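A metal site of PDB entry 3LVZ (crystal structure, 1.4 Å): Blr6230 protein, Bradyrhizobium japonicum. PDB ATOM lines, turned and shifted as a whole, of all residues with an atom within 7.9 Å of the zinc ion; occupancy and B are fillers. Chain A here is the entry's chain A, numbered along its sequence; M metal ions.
OE1 of Glu 158 sits at hydrogen-bond distance from N of Ala 173 (2.8 Å). NE2 of His 172 lies within hydrogen-bond range of OE1 of Glu 185 (3.2 Å). O of Ser 183 sits at hydrogen-bond distance from N of His 172, at 2.8 Å.
Met 233 touches the zinc ion. Within 4 Å of the zinc ion: Glu 158, His 172, Lys 229 and Met 233.
The zinc ion is bound by OE2 of Glu 158. NZ of Lys 229 is bound to the zinc ion, at 2.0 Å. The zinc ion is bound by ND1 of His 172 (2.1 Å). The zinc ion has three donor atoms within binding distance.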
ATOM      1  N   GLU A 158     -16.671  -9.039 -24.194  1.00  0.00           N
ATOM      2  CA  GLU A 158     -16.768  -7.992 -23.209  1.00  0.00           C
ATOM      3  C   GLU A 158     -16.313  -8.506 -21.858  1.00  0.00           C
ATOM      4  O   GLU A 158     -16.732  -9.594 -21.362  1.00  0.00           O
ATOM      5  CB  GLU A 158     -18.252  -7.532 -23.058  1.00  0.00           C
ATOM      6  CG  GLU A 158     -18.494  -6.682 -21.844  1.00  0.00           C
ATOM      7  CD  GLU A 158     -17.948  -5.303 -21.966  1.00  0.00           C
ATOM      8  OE1 GLU A 158     -17.748  -4.743 -23.046  1.00  0.00           O
ATOM      9  OE2 GLU A 158     -17.949  -4.607 -20.916  1.00  0.00           O
ATOM     10  N   GLY A 159     -15.404  -7.728 -21.220  1.00  0.00           N
ATOM     11  CA  GLY A 159     -14.936  -8.042 -19.885  1.00  0.00           C
ATOM     12  C   GLY A 159     -13.755  -8.999 -19.773  1.00  0.00           C
ATOM     13  O   GLY A 159     -13.199  -9.174 -18.671  1.00  0.00           O
ATOM     14  N   THR A 170      -8.430  -4.853 -20.204  1.00  0.00           N
ATOM     15  CA  THR A 170      -9.764  -5.408 -20.207  1.00  0.00           C
ATOM     16  C   THR A 170     -10.404  -5.034 -21.491  1.00  0.00           C
ATOM     17  O   THR A 170     -10.395  -3.886 -21.929  1.00  0.00           O
ATOM     18  CB  THR A 170     -10.553  -4.918 -18.979  1.00  0.00           C
ATOM     19  OG1 THR A 170      -9.910  -5.334 -17.781  1.00  0.00           O
ATOM     20  CG2 THR A 170     -11.983  -5.385 -19.023  1.00  0.00           C
ATOM     21  N   ALA A 171     -11.027  -6.050 -22.145  1.00  0.00           N
ATOM     22  CA  ALA A 171     -11.717  -5.859 -23.405  1.00  0.00           C
ATOM     23  C   ALA A 171     -13.109  -5.294 -23.181  1.00  0.00           C
ATOM     24  O   ALA A 171     -13.867  -5.773 -22.292  1.00  0.00           O
ATOM     25  CB  ALA A 171     -11.863  -7.195 -24.161  1.00  0.00           C
ATOM     26  N   HIS A 172     -13.469  -4.281 -23.959  1.00  0.00           N
ATOM     27  CA  HIS A 172     -14.821  -3.741 -24.034  1.00  0.00           C
ATOM     28  C   HIS A 172     -15.380  -3.816 -25.440  1.00  0.00           C
ATOM     29  O   HIS A 172     -14.735  -3.359 -26.372  1.00  0.00           O
ATOM     30  CB  HIS A 172     -14.877  -2.335 -23.540  1.00  0.00           C
ATOM     31  CG  HIS A 172     -14.505  -2.182 -22.116  1.00  0.00           C
ATOM     32  ND1 HIS A 172     -15.443  -2.292 -21.135  1.00  0.00           N
ATOM     33  CD2 HIS A 172     -13.325  -1.976 -21.500  1.00  0.00           C
ATOM     34  CE1 HIS A 172     -14.862  -2.131 -19.944  1.00  0.00           C
ATOM     35  NE2 HIS A 172     -13.571  -1.975 -20.138  1.00  0.00           N
ATOM     36  N   ALA A 173     -16.532  -4.492 -25.574  1.00  0.00           N
ATOM     37  CA  ALA A 173     -17.120  -4.668 -26.894  1.00  0.00           C
ATOM     38  C   ALA A 173     -17.789  -3.350 -27.282  1.00  0.00           C
ATOM     39  O   ALA A 173     -18.821  -2.931 -26.705  1.00  0.00           O
ATOM     40  CB  ALA A 173     -18.136  -5.855 -26.897  1.00  0.00           C
ATOM     41  N   THR A 174     -17.329  -2.723 -28.320  1.00  0.00           N
ATOM     42  CA  THR A 174     -17.764  -1.383 -28.780  1.00  0.00           C
ATOM     43  C   THR A 174     -17.862  -1.462 -30.310  1.00  0.00           C
ATOM     44  O   THR A 174     -17.286  -0.629 -31.046  1.00  0.00           O
ATOM     45  CB  THR A 174     -16.807  -0.233 -28.345  1.00  0.00           C
ATOM     46  OG1 THR A 174     -15.484  -0.580 -28.668  1.00  0.00           O
ATOM     47  CG2 THR A 174     -16.872  -0.084 -26.802  1.00  0.00           C
ATOM     48  N   SER A 183     -12.490  -1.952 -27.550  1.00  0.00           N
ATOM     49  CA  SER A 183     -11.813  -0.866 -26.848  1.00  0.00           C
ATOM     50  C   SER A 183     -11.170  -1.485 -25.629  1.00  0.00           C
ATOM     51  O   SER A 183     -11.739  -2.329 -24.924  1.00  0.00           O
ATOM     52  CB  SER A 183     -12.830   0.212 -26.424  1.00  0.00           C
ATOM     53  OG  SER A 183     -13.354   0.839 -27.554  1.00  0.00           O
ATOM     54  N   GLU A 185      -9.154  -1.306 -21.964  1.00  0.00           N
ATOM     55  CA  GLU A 185      -8.921  -0.471 -20.790  1.00  0.00           C
ATOM     56  C   GLU A 185      -7.760  -0.987 -19.957  1.00  0.00           C
ATOM     57  O   GLU A 185      -7.588  -2.179 -19.800  1.00  0.00           O
ATOM     58  CB  GLU A 185     -10.172  -0.445 -19.990  1.00  0.00           C
ATOM     59  CG  GLU A 185     -10.107   0.481 -18.796  1.00  0.00           C
ATOM     60  CD  GLU A 185     -11.448   0.831 -18.162  1.00  0.00           C
ATOM     61  OE1 GLU A 185     -12.535   0.792 -18.825  1.00  0.00           O
ATOM     62  OE2 GLU A 185     -11.360   1.294 -16.995  1.00  0.00           O
ATOM     63  N   LEU A 198      -8.144   4.335 -21.974  1.00  0.00           N
ATOM     64  CA  LEU A 198      -8.939   3.549 -22.893  1.00  0.00           C
ATOM     65  C   LEU A 198      -8.338   3.663 -24.282  1.00  0.00           C
ATOM     66  O   LEU A 198      -8.264   4.797 -24.786  1.00  0.00           O
ATOM     67  CB  LEU A 198     -10.398   3.978 -23.023  1.00  0.00           C
ATOM     68  CG  LEU A 198     -11.268   2.985 -23.795  1.00  0.00           C
ATOM     69  CD1 LEU A 198     -11.467   1.690 -23.025  1.00  0.00           C
ATOM     70  CD2 LEU A 198     -12.535   3.695 -24.235  1.00  0.00           C
ATOM     71  N   LYS A 229     -22.368   3.607 -24.466  1.00  0.00           N
ATOM     72  CA  LYS A 229     -21.376   2.929 -23.656  1.00  0.00           C
ATOM     73  C   LYS A 229     -20.179   3.852 -23.438  1.00  0.00           C
ATOM     74  O   LYS A 229     -19.694   4.018 -22.275  1.00  0.00           O
ATOM     75  CB  LYS A 229     -20.921   1.680 -24.415  1.00  0.00           C
ATOM     76  CG  LYS A 229     -20.002   0.858 -23.622  1.00  0.00           C
ATOM     77  CD  LYS A 229     -19.708  -0.449 -24.281  1.00  0.00           C
ATOM     78  CE  LYS A 229     -18.524  -1.051 -23.557  1.00  0.00           C
ATOM     79  NZ  LYS A 229     -18.694  -1.760 -22.394  1.00  0.00           N
ATOM     80  N   MET A 233     -18.394   5.375 -19.532  1.00  0.00           N
ATOM     81  CA  MET A 233     -17.101   4.918 -18.989  1.00  0.00           C
ATOM     82  C   MET A 233     -16.393   6.075 -18.283  1.00  0.00           C
ATOM     83  O   MET A 233     -16.632   7.247 -18.554  1.00  0.00           O
ATOM     84  CB  MET A 233     -16.219   4.345 -20.096  1.00  0.00           C
ATOM     85  CG  MET A 233     -16.849   3.141 -20.774  1.00  0.00           C
ATOM     86  SD  MET A 233     -15.849   2.621 -22.153  1.00  0.00           S
ATOM     87  CE  MET A 233     -16.324   0.957 -22.263  1.00  0.00           C
HETATM   88 ZN    ZN M   1     -17.475  -2.676 -21.077  1.00  0.00          ZN
